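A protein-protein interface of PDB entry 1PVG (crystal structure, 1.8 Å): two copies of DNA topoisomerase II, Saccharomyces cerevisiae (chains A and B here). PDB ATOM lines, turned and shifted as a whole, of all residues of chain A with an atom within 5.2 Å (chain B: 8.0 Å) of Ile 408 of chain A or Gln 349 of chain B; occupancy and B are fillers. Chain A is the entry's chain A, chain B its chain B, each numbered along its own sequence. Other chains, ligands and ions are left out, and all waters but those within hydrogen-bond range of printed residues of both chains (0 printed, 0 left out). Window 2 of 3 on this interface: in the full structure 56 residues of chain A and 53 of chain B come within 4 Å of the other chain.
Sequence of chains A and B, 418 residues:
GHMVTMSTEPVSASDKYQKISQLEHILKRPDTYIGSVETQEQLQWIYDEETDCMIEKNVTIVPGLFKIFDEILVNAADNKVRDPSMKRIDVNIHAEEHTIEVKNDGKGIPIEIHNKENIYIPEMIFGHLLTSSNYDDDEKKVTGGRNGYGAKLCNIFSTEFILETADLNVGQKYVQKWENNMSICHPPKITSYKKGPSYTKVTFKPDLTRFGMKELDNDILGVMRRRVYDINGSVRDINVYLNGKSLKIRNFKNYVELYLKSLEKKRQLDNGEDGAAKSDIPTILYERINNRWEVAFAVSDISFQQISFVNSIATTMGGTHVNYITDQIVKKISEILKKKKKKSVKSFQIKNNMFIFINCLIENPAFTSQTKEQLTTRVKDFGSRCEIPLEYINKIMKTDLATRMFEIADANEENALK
Hydrophobic or aromatic side chains of chain A that line the printed part of chain B: Phe 348 and Ile 408. Of the 21 printed residues of chain B, 4 touch a printed residue of chain A. Hydrophobic or aromatic side chains of chain B that line the printed part of chain A: Phe 348. Among the printed residues, 6 pairs touch across the chains.
Phe 348 of chain B touches its own counterpart, Phe 348 of chain A. Phe 348 of chain A touches Gln 349 of chain B, but with the chains exchanged Gln 349 of chain A does not touch Phe 348 of chain B (4.1 Å). Gln 349 of chain A touches its own counterpart, Gln 349 of chain B. Ile 408 of chain A touches Gln 349 of chain B, but with the chains exchanged Gln 349 of chain A does not touch Ile 408 of chain B (4.6 Å). Positions printed for both chains: 345, 348, 349, 404, 405, 407, 408 and 409. Of the 6 pairs that touch across the chains among the printed residues, 2 have their exchanged pair printed and touching as well.
The backbone NH of Phe 304 of chain B is in hydrogen-bond range of the side-chain amide oxygen of Asn 352 of chain B. The side-chain amide nitrogen (ND2) of Asn 352 of chain B lies within hydrogen-bond range of the backbone carbonyl oxygen (O) of Phe 348 of chain B, at 3.1 Å. The backbone carbonyl oxygen (O) of Gln 349 of chain B sits at hydrogen-bond distance from the side-chain amide nitrogen (ND2) of Asn 353 of chain B (2.7 Å).
Among the printed residues, merely in contact across the chains: Phe 348 of chain A with Phe 348 of chain B, Phe 348 of chain A with Gln 349 of chain B, Phe 348 of chain A with Asn 352 of chain B, Arg 404 of chain A with Lys 346 of chain B and Ile 408 of chain A with Gln 349 of chain B.
Printed residues of chain B within 4 Å of Phe 348 of chain A: Phe 348 (3.7 Å), Gln 349 (3.6 Å) and Asn 352 (3.6 Å). Printed residues of chain B within 4 Å of Gln 349 of chain A: Gln 349 (3.2 Å). Ile 408 of chain A touches just one residue of chain B: Gln 349. No residue of chain B comes within 4 Å of Ala 409 of chain A. Asp 410 of chain A touches none of the printed residues of chain B. Of the printed residues of chain A, Lys 346 of chain B touches Arg 404 (3.8 Å). Of the printed residues of chain A, Phe 348 of chain B touches Phe 348. Of chain A, only Phe 348, Gln 349 and Ile 408 come within 4 Å of Gln 349 of chain B. Of the printed residues of chain A, Asn 352 of chain B touches Phe 348. The nearest residue of chain B that does not touch Ile 408 of chain A is Ile 408 of chain B (5.9 Å). The nearest printed residue of chain A that does not touch Gln 349 of chain B is Met 405 of chain A (6.7 Å). The nearest printed residue of chain A that does not touch Lys 346 of chain B is Met 405 of chain A (6.7 Å).
The side-chain amide oxygen (OE1) of Gln 349 of chain A sits close to the side-chain amide oxygen (OE1) of Gln 349 of chain B (3.2 Å).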
ATOM      1  N   VAL A 345      25.277 -19.826  17.294  1.00  0.00           N
ATOM      2  CA  VAL A 345      25.985 -18.628  17.733  1.00  0.00           C
ATOM      3  C   VAL A 345      27.493 -18.874  17.747  1.00  0.00           C
ATOM      4  O   VAL A 345      27.938 -20.021  17.859  1.00  0.00           O
ATOM      5  CB  VAL A 345      25.492 -18.136  19.129  1.00  0.00           C
ATOM      6  CG1 VAL A 345      23.989 -18.322  19.272  1.00  0.00           C
ATOM      7  CG2 VAL A 345      26.238 -18.835  20.271  1.00  0.00           C
ATOM      8  N   PHE A 348      32.964 -17.276  20.515  1.00  0.00           N
ATOM      9  CA  PHE A 348      33.429 -16.142  21.321  1.00  0.00           C
ATOM     10  C   PHE A 348      32.309 -15.441  22.106  1.00  0.00           C
ATOM     11  O   PHE A 348      32.556 -14.837  23.151  1.00  0.00           O
ATOM     12  CB  PHE A 348      34.240 -15.137  20.474  1.00  0.00           C
ATOM     13  CG  PHE A 348      33.398 -14.198  19.640  1.00  0.00           C
ATOM     14  CD1 PHE A 348      32.695 -13.142  20.228  1.00  0.00           C
ATOM     15  CD2 PHE A 348      33.345 -14.344  18.260  1.00  0.00           C
ATOM     16  CE1 PHE A 348      31.936 -12.285  19.466  1.00  0.00           C
ATOM     17  CE2 PHE A 348      32.596 -13.485  17.485  1.00  0.00           C
ATOM     18  CZ  PHE A 348      31.883 -12.447  18.084  1.00  0.00           C
ATOM     19  N   GLN A 349      31.087 -15.525  21.591  1.00  0.00           N
ATOM     20  CA  GLN A 349      29.915 -14.969  22.268  1.00  0.00           C
ATOM     21  C   GLN A 349      29.594 -15.715  23.563  1.00  0.00           C
ATOM     22  O   GLN A 349      29.252 -15.097  24.578  1.00  0.00           O
ATOM     23  CB  GLN A 349      28.712 -14.952  21.323  1.00  0.00           C
ATOM     24  CG  GLN A 349      28.904 -13.995  20.159  1.00  0.00           C
ATOM     25  CD  GLN A 349      27.772 -14.015  19.165  1.00  0.00           C
ATOM     26  OE1 GLN A 349      27.352 -12.957  18.679  1.00  0.00           O
ATOM     27  NE2 GLN A 349      27.278 -15.208  18.840  1.00  0.00           N
ATOM     28  N   ARG A 404      21.041 -14.849  27.591  1.00  0.00           N
ATOM     29  CA  ARG A 404      21.838 -13.968  26.747  1.00  0.00           C
ATOM     30  C   ARG A 404      22.116 -14.634  25.395  1.00  0.00           C
ATOM     31  O   ARG A 404      22.044 -13.985  24.355  1.00  0.00           O
ATOM     32  CB  ARG A 404      23.151 -13.592  27.435  1.00  0.00           C
ATOM     33  CG  ARG A 404      23.033 -12.487  28.473  1.00  0.00           C
ATOM     34  CD  ARG A 404      24.330 -12.233  29.209  1.00  0.00           C
ATOM     35  NE  ARG A 404      24.160 -11.637  30.532  1.00  0.00           N
ATOM     36  CZ  ARG A 404      25.172 -11.318  31.336  1.00  0.00           C
ATOM     37  NH1 ARG A 404      26.425 -11.538  30.952  1.00  0.00           N
ATOM     38  NH2 ARG A 404      24.938 -10.776  32.524  1.00  0.00           N
ATOM     39  N   MET A 405      22.402 -15.937  25.419  1.00  0.00           N
ATOM     40  CA  MET A 405      22.673 -16.686  24.195  1.00  0.00           C
ATOM     41  C   MET A 405      21.411 -16.881  23.343  1.00  0.00           C
ATOM     42  O   MET A 405      21.486 -16.872  22.113  1.00  0.00           O
ATOM     43  CB  MET A 405      23.333 -18.036  24.501  1.00  0.00           C
ATOM     44  CG  MET A 405      24.798 -17.959  25.006  1.00  0.00           C
ATOM     45  SD  MET A 405      25.977 -16.700  24.055  1.00  0.00           S
ATOM     46  CE  MET A 405      25.679 -15.132  25.137  1.00  0.00           C
ATOM     47  N   PHE A 406      20.262 -17.055  24.001  1.00  0.00           N
ATOM     48  CA  PHE A 406      18.976 -17.183  23.303  1.00  0.00           C
ATOM     49  C   PHE A 406      18.588 -15.872  22.625  1.00  0.00           C
ATOM     50  O   PHE A 406      17.979 -15.869  21.551  1.00  0.00           O
ATOM     51  CB  PHE A 406      17.864 -17.608  24.271  1.00  0.00           C
ATOM     52  CG  PHE A 406      18.069 -18.968  24.892  1.00  0.00           C
ATOM     53  CD1 PHE A 406      18.745 -19.978  24.206  1.00  0.00           C
ATOM     54  CD2 PHE A 406      17.566 -19.245  26.163  1.00  0.00           C
ATOM     55  CE1 PHE A 406      18.933 -21.233  24.785  1.00  0.00           C
ATOM     56  CE2 PHE A 406      17.745 -20.499  26.748  1.00  0.00           C
ATOM     57  CZ  PHE A 406      18.431 -21.494  26.057  1.00  0.00           C
ATOM     58  N   GLU A 407      18.936 -14.762  23.272  1.00  0.00           N
ATOM     59  CA  GLU A 407      18.731 -13.426  22.717  1.00  0.00           C
ATOM     60  C   GLU A 407      19.500 -13.242  21.407  1.00  0.00           C
ATOM     61  O   GLU A 407      18.970 -12.695  20.440  1.00  0.00           O
ATOM     62  CB  GLU A 407      19.167 -12.369  23.730  1.00  0.00           C
ATOM     63  CG  GLU A 407      18.243 -11.169  23.820  1.00  0.00           C
ATOM     64  CD  GLU A 407      18.418 -10.407  25.116  1.00  0.00           C
ATOM     65  OE1 GLU A 407      19.560  -9.995  25.416  1.00  0.00           O
ATOM     66  OE2 GLU A 407      17.414 -10.223  25.838  1.00  0.00           O
ATOM     67  N   ILE A 408      20.751 -13.704  21.383  1.00  0.00           N
ATOM     68  CA  ILE A 408      21.568 -13.657  20.172  1.00  0.00           C
ATOM     69  C   ILE A 408      21.041 -14.632  19.111  1.00  0.00           C
ATOM     70  O   ILE A 408      20.980 -14.295  17.925  1.00  0.00           O
ATOM     71  CB  ILE A 408      23.058 -13.936  20.503  1.00  0.00           C
ATOM     72  CG1 ILE A 408      23.671 -12.737  21.237  1.00  0.00           C
ATOM     73  CG2 ILE A 408      23.852 -14.261  19.231  1.00  0.00           C
ATOM     74  CD1 ILE A 408      25.036 -13.011  21.866  1.00  0.00           C
ATOM     75  N   ALA A 409      20.643 -15.826  19.551  1.00  0.00           N
ATOM     76  CA  ALA A 409      20.135 -16.864  18.652  1.00  0.00           C
ATOM     77  C   ALA A 409      18.887 -16.421  17.880  1.00  0.00           C
ATOM     78  O   ALA A 409      18.790 -16.646  16.668  1.00  0.00           O
ATOM     79  CB  ALA A 409      19.860 -18.149  19.423  1.00  0.00           C
ATOM     80  N   ASP A 410      17.945 -15.791  18.583  1.00  0.00           N
ATOM     81  CA  ASP A 410      16.692 -15.327  17.975  1.00  0.00           C
ATOM     82  C   ASP A 410      16.944 -14.259  16.909  1.00  0.00           C
ATOM     83  O   ASP A 410      16.316 -14.265  15.850  1.00  0.00           O
ATOM     84  CB  ASP A 410      15.730 -14.798  19.046  1.00  0.00           C
ATOM     85  CG  ASP A 410      15.233 -15.893  19.984  1.00  0.00           C
ATOM     86  OD1 ASP A 410      15.258 -17.081  19.596  1.00  0.00           O
ATOM     87  OD2 ASP A 410      14.796 -15.655  21.131  1.00  0.00           O
ATOM     88  N   ALA A 411      17.873 -13.352  17.200  1.00  0.00           N
ATOM     89  CA  ALA A 411      18.328 -12.361  16.229  1.00  0.00           C
ATOM     90  C   ALA A 411      19.643 -12.790  15.580  1.00  0.00           C
ATOM     91  O   ALA A 411      19.670 -13.692  14.733  1.00  0.00           O
ATOM     92  CB  ALA A 411      18.485 -11.004  16.896  1.00  0.00           C
ATOM     93  N   PHE B 304      38.638 -12.592  16.831  1.00  0.00           N
ATOM     94  CA  PHE B 304      39.724 -11.626  16.648  1.00  0.00           C
ATOM     95  C   PHE B 304      40.965 -12.309  16.088  1.00  0.00           C
ATOM     96  O   PHE B 304      41.360 -13.382  16.554  1.00  0.00           O
ATOM     97  CB  PHE B 304      40.062 -10.918  17.967  1.00  0.00           C
ATOM     98  CG  PHE B 304      41.267 -10.026  17.882  1.00  0.00           C
ATOM     99  CD1 PHE B 304      41.240  -8.872  17.104  1.00  0.00           C
ATOM    100  CD2 PHE B 304      42.445 -10.352  18.558  1.00  0.00           C
ATOM    101  CE1 PHE B 304      42.369  -8.041  17.013  1.00  0.00           C
ATOM    102  CE2 PHE B 304      43.577  -9.535  18.473  1.00  0.00           C
ATOM    103  CZ  PHE B 304      43.536  -8.374  17.706  1.00  0.00           C
ATOM    104  N   VAL B 330      38.255  -0.030  18.567  1.00  0.00           N
ATOM    105  CA  VAL B 330      37.107  -0.542  19.324  1.00  0.00           C
ATOM    106  C   VAL B 330      36.434   0.584  20.124  1.00  0.00           C
ATOM    107  O   VAL B 330      35.209   0.681  20.150  1.00  0.00           O
ATOM    108  CB  VAL B 330      37.509  -1.723  20.256  1.00  0.00           C
ATOM    109  CG1 VAL B 330      36.363  -2.108  21.184  1.00  0.00           C
ATOM    110  CG2 VAL B 330      37.943  -2.930  19.427  1.00  0.00           C
ATOM    111  N   ILE B 333      34.369   2.785  17.600  1.00  0.00           N
ATOM    112  CA  ILE B 333      33.221   2.038  17.100  1.00  0.00           C
ATOM    113  C   ILE B 333      32.149   1.901  18.183  1.00  0.00           C
ATOM    114  O   ILE B 333      30.957   2.036  17.899  1.00  0.00           O
ATOM    115  CB  ILE B 333      33.644   0.661  16.522  1.00  0.00           C
ATOM    116  CG1 ILE B 333      34.511   0.871  15.271  1.00  0.00           C
ATOM    117  CG2 ILE B 333      32.400  -0.198  16.193  1.00  0.00           C
ATOM    118  CD1 ILE B 333      35.208  -0.374  14.755  1.00  0.00           C
ATOM    119  N   LEU B 337      28.172   3.190  17.928  1.00  0.00           N
ATOM    120  CA  LEU B 337      27.046   2.288  18.152  1.00  0.00           C
ATOM    121  C   LEU B 337      26.166   2.747  19.311  1.00  0.00           C
ATOM    122  O   LEU B 337      24.952   2.546  19.290  1.00  0.00           O
ATOM    123  CB  LEU B 337      27.537   0.858  18.398  1.00  0.00           C
ATOM    124  CG  LEU B 337      28.308   0.186  17.257  1.00  0.00           C
ATOM    125  CD1 LEU B 337      28.966  -1.104  17.736  1.00  0.00           C
ATOM    126  CD2 LEU B 337      27.401  -0.076  16.064  1.00  0.00           C
ATOM    127  N   SER B 344      24.438  -1.248  24.594  1.00  0.00           N
ATOM    128  CA  SER B 344      23.800  -2.315  23.828  1.00  0.00           C
ATOM    129  C   SER B 344      24.820  -3.304  23.255  1.00  0.00           C
ATOM    130  O   SER B 344      24.584  -4.515  23.258  1.00  0.00           O
ATOM    131  CB  SER B 344      22.925  -1.731  22.716  1.00  0.00           C
ATOM    132  N   VAL B 345      25.949  -2.785  22.767  1.00  0.00           N
ATOM    133  CA  VAL B 345      26.998  -3.621  22.171  1.00  0.00           C
ATOM    134  C   VAL B 345      28.269  -3.617  23.018  1.00  0.00           C
ATOM    135  O   VAL B 345      28.887  -2.570  23.218  1.00  0.00           O
ATOM    136  CB  VAL B 345      27.357  -3.177  20.724  1.00  0.00           C
ATOM    137  CG1 VAL B 345      28.438  -4.079  20.143  1.00  0.00           C
ATOM    138  CG2 VAL B 345      26.130  -3.185  19.830  1.00  0.00           C
ATOM    139  N   LYS B 346      28.664  -4.797  23.496  1.00  0.00           N
ATOM    140  CA  LYS B 346      29.891  -4.946  24.274  1.00  0.00           C
ATOM    141  C   LYS B 346      31.141  -4.927  23.386  1.00  0.00           C
ATOM    142  O   LYS B 346      31.116  -5.390  22.244  1.00  0.00           O
ATOM    143  CB  LYS B 346      29.850  -6.232  25.114  1.00  0.00           C
ATOM    144  CG  LYS B 346      28.757  -6.249  26.180  1.00  0.00           C
ATOM    145  CD  LYS B 346      28.772  -7.540  26.977  1.00  0.00           C
ATOM    146  CE  LYS B 346      27.373  -8.077  27.195  1.00  0.00           C
ATOM    147  NZ  LYS B 346      27.392  -9.346  27.976  1.00  0.00           N
ATOM    148  N   SER B 347      32.228  -4.384  23.925  1.00  0.00           N
ATOM    149  CA  SER B 347      33.487  -4.257  23.190  1.00  0.00           C
ATOM    150  C   SER B 347      33.963  -5.553  22.538  1.00  0.00           C
ATOM    151  O   SER B 347      34.462  -5.521  21.415  1.00  0.00           O
ATOM    152  CB  SER B 347      34.588  -3.678  24.089  1.00  0.00           C
ATOM    153  OG  SER B 347      34.350  -2.295  24.335  1.00  0.00           O
ATOM    154  N   PHE B 348      33.810  -6.691  23.228  1.00  0.00           N
ATOM    155  CA  PHE B 348      34.299  -7.964  22.684  1.00  0.00           C
ATOM    156  C   PHE B 348      33.640  -8.320  21.350  1.00  0.00           C
ATOM    157  O   PHE B 348      34.262  -8.924  20.489  1.00  0.00           O
ATOM    158  CB  PHE B 348      34.191  -9.121  23.702  1.00  0.00           C
ATOM    159  CG  PHE B 348      32.805  -9.689  23.856  1.00  0.00           C
ATOM    160  CD1 PHE B 348      32.288 -10.580  22.914  1.00  0.00           C
ATOM    161  CD2 PHE B 348      32.034  -9.376  24.973  1.00  0.00           C
ATOM    162  CE1 PHE B 348      31.017 -11.123  23.065  1.00  0.00           C
ATOM    163  CE2 PHE B 348      30.760  -9.915  25.131  1.00  0.00           C
ATOM    164  CZ  PHE B 348      30.250 -10.791  24.178  1.00  0.00           C
ATOM    165  N   GLN B 349      32.387  -7.909  21.179  1.00  0.00           N
ATOM    166  CA  GLN B 349      31.654  -8.197  19.949  1.00  0.00           C
ATOM    167  C   GLN B 349      32.299  -7.474  18.770  1.00  0.00           C
ATOM    168  O   GLN B 349      32.382  -8.019  17.660  1.00  0.00           O
ATOM    169  CB  GLN B 349      30.184  -7.805  20.092  1.00  0.00           C
ATOM    170  CG  GLN B 349      29.429  -8.605  21.162  1.00  0.00           C
ATOM    171  CD  GLN B 349      28.570  -9.701  20.572  1.00  0.00           C
ATOM    172  OE1 GLN B 349      28.925 -10.293  19.546  1.00  0.00           O
ATOM    173  NE2 GLN B 349      27.436  -9.976  21.209  1.00  0.00           N
ATOM    174  N   ILE B 350      32.767  -6.252  19.023  1.00  0.00           N
ATOM    175  CA  ILE B 350      33.465  -5.463  18.014  1.00  0.00           C
ATOM    176  C   ILE B 350      34.819  -6.078  17.716  1.00  0.00           C
ATOM    177  O   ILE B 350      35.133  -6.382  16.564  1.00  0.00           O
ATOM    178  CB  ILE B 350      33.645  -3.996  18.481  1.00  0.00           C
ATOM    179  CG1 ILE B 350      32.292  -3.372  18.819  1.00  0.00           C
ATOM    180  CG2 ILE B 350      34.384  -3.164  17.396  1.00  0.00           C
ATOM    181  CD1 ILE B 350      32.383  -2.103  19.642  1.00  0.00           C
ATOM    182  N   LYS B 351      35.616  -6.284  18.760  1.00  0.00           N
ATOM    183  CA  LYS B 351      36.972  -6.791  18.574  1.00  0.00           C
ATOM    184  C   LYS B 351      37.005  -8.140  17.831  1.00  0.00           C
ATOM    185  O   LYS B 351      37.863  -8.362  16.970  1.00  0.00           O
ATOM    186  CB  LYS B 351      37.702  -6.904  19.917  1.00  0.00           C
ATOM    187  CG  LYS B 351      39.179  -7.216  19.755  1.00  0.00           C
ATOM    188  CD  LYS B 351      39.894  -7.384  21.084  1.00  0.00           C
ATOM    189  CE  LYS B 351      41.396  -7.517  20.845  1.00  0.00           C
ATOM    190  NZ  LYS B 351      42.130  -7.894  22.082  1.00  0.00           N
ATOM    191  N   ASN B 352      36.078  -9.035  18.164  1.00  0.00           N
ATOM    192  CA  ASN B 352      36.086 -10.366  17.578  1.00  0.00           C
ATOM    193  C   ASN B 352      35.579 -10.451  16.134  1.00  0.00           C
ATOM    194  O   ASN B 352      35.468 -11.538  15.571  1.00  0.00           O
ATOM    195  CB  ASN B 352      35.390 -11.376  18.496  1.00  0.00           C
ATOM    196  CG  ASN B 352      36.302 -11.855  19.613  1.00  0.00           C
ATOM    197  OD1 ASN B 352      37.250 -12.599  19.367  1.00  0.00           O
ATOM    198  ND2 ASN B 352      36.046 -11.398  20.834  1.00  0.00           N
ATOM    199  N   ASN B 353      35.264  -9.304  15.541  1.00  0.00           N
ATOM    200  CA  ASN B 353      35.023  -9.260  14.113  1.00  0.00           C
ATOM    201  C   ASN B 353      36.165  -8.584  13.353  1.00  0.00           C
ATOM    202  O   ASN B 353      36.022  -8.264  12.176  1.00  0.00           O
ATOM    203  CB  ASN B 353      33.675  -8.595  13.825  1.00  0.00           C
ATOM    204  CG  ASN B 353      32.505  -9.505  14.146  1.00  0.00           C
ATOM    205  OD1 ASN B 353      32.136 -10.365  13.346  1.00  0.00           O
ATOM    206  ND2 ASN B 353      31.932  -9.337  15.328  1.00  0.00           N
ATOM    207  N   MET B 354      37.307  -8.408  14.024  1.00  0.00           N
ATOM    208  CA  MET B 354      38.457  -7.699  13.452  1.00  0.00           C
ATOM    209  C   MET B 354      39.640  -8.616  13.148  1.00  0.00           C
ATOM    210  O   MET B 354      39.977  -9.496  13.949  1.00  0.00           O
ATOM    211  CB  MET B 354      38.940  -6.594  14.396  1.00  0.00           C
ATOM    212  CG  MET B 354      37.917  -5.518  14.718  1.00  0.00           C
ATOM    213  SD  MET B 354      38.704  -4.154  15.894  1.00  0.00           S
ATOM    214  CE  MET B 354      40.492  -3.991  14.963  1.00  0.00           C
ATOM    215  N   LEU B 401      31.756  -5.430   9.246  1.00  0.00           N
ATOM    216  CA  LEU B 401      31.807  -5.275  10.699  1.00  0.00           C
ATOM    217  C   LEU B 401      30.623  -4.463  11.212  1.00  0.00           C
ATOM    218  O   LEU B 401      29.969  -4.860  12.175  1.00  0.00           O
ATOM    219  CB  LEU B 401      33.128  -4.636  11.144  1.00  0.00           C
ATOM    220  CG  LEU B 401      33.405  -4.679  12.650  1.00  0.00           C
ATOM    221  CD1 LEU B 401      34.867  -5.010  12.928  1.00  0.00           C
ATOM    222  CD2 LEU B 401      33.027  -3.370  13.310  1.00  0.00           C
ATOM    223  N   ARG B 404      27.208  -6.181  10.933  1.00  0.00           N
ATOM    224  CA  ARG B 404      27.117  -7.158  12.013  1.00  0.00           C
ATOM    225  C   ARG B 404      26.840  -6.487  13.361  1.00  0.00           C
ATOM    226  O   ARG B 404      26.101  -7.028  14.188  1.00  0.00           O
ATOM    227  CB  ARG B 404      28.405  -7.975  12.102  1.00  0.00           C
ATOM    228  CG  ARG B 404      28.600  -8.980  10.987  1.00  0.00           C
ATOM    229  CD  ARG B 404      29.998  -9.534  10.932  1.00  0.00           C
ATOM    230  NE  ARG B 404      30.292 -10.218   9.677  1.00  0.00           N
ATOM    231  CZ  ARG B 404      31.346 -11.007   9.492  1.00  0.00           C
ATOM    232  NH1 ARG B 404      32.204 -11.215  10.482  1.00  0.00           N
ATOM    233  NH2 ARG B 404      31.545 -11.590   8.317  1.00  0.00           N
ATOM    234  N   MET B 405      27.444  -5.314  13.574  1.00  0.00           N
ATOM    235  CA  MET B 405      27.304  -4.580  14.838  1.00  0.00           C
ATOM    236  C   MET B 405      25.948  -3.886  14.959  1.00  0.00           C
ATOM    237  O   MET B 405      25.446  -3.675  16.065  1.00  0.00           O
ATOM    238  CB  MET B 405      28.433  -3.556  15.004  1.00  0.00           C
ATOM    239  CG  MET B 405      29.809  -4.152  15.294  1.00  0.00           C
ATOM    240  SD  MET B 405      29.781  -5.525  16.667  1.00  0.00           S
ATOM    241  CE  MET B 405      29.657  -7.103  15.521  1.00  0.00           C
ATOM    242  N   GLU B 407      23.229  -5.167  13.729  1.00  0.00           N
ATOM    243  CA  GLU B 407      22.269  -6.252  13.918  1.00  0.00           C
ATOM    244  C   GLU B 407      22.146  -6.637  15.396  1.00  0.00           C
ATOM    245  O   GLU B 407      21.066  -7.014  15.858  1.00  0.00           O
ATOM    246  CB  GLU B 407      22.664  -7.470  13.078  1.00  0.00           C
ATOM    247  CG  GLU B 407      22.196  -7.399  11.630  1.00  0.00           C
ATOM    248  CD  GLU B 407      22.863  -8.424  10.726  1.00  0.00           C
ATOM    249  OE1 GLU B 407      23.814  -9.107  11.174  1.00  0.00           O
ATOM    250  OE2 GLU B 407      22.434  -8.544   9.555  1.00  0.00           O
ATOM    251  N   ILE B 408      23.255  -6.535  16.129  1.00  0.00           N
ATOM    252  CA  ILE B 408      23.274  -6.817  17.566  1.00  0.00           C
ATOM    253  C   ILE B 408      22.589  -5.688  18.347  1.00  0.00           C
ATOM    254  O   ILE B 408      21.788  -5.946  19.250  1.00  0.00           O
ATOM    255  CB  ILE B 408      24.735  -7.047  18.068  1.00  0.00           C
ATOM    256  CG1 ILE B 408      25.279  -8.380  17.538  1.00  0.00           C
ATOM    257  CG2 ILE B 408      24.808  -7.009  19.595  1.00  0.00           C
ATOM    258  CD1 ILE B 408      26.794  -8.503  17.592  1.00  0.00           C
ATOM    259  N   ALA B 409      22.901  -4.445  17.983  1.00  0.00           N
ATOM    260  CA  ALA B 409      22.273  -3.271  18.595  1.00  0.00           C
ATOM    261  C   ALA B 409      20.799  -3.152  18.201  1.00  0.00           C
ATOM    262  O   ALA B 409      19.923  -3.072  19.067  1.00  0.00           O
ATOM    263  CB  ALA B 409      23.034  -2.001  18.216  1.00  0.00           C
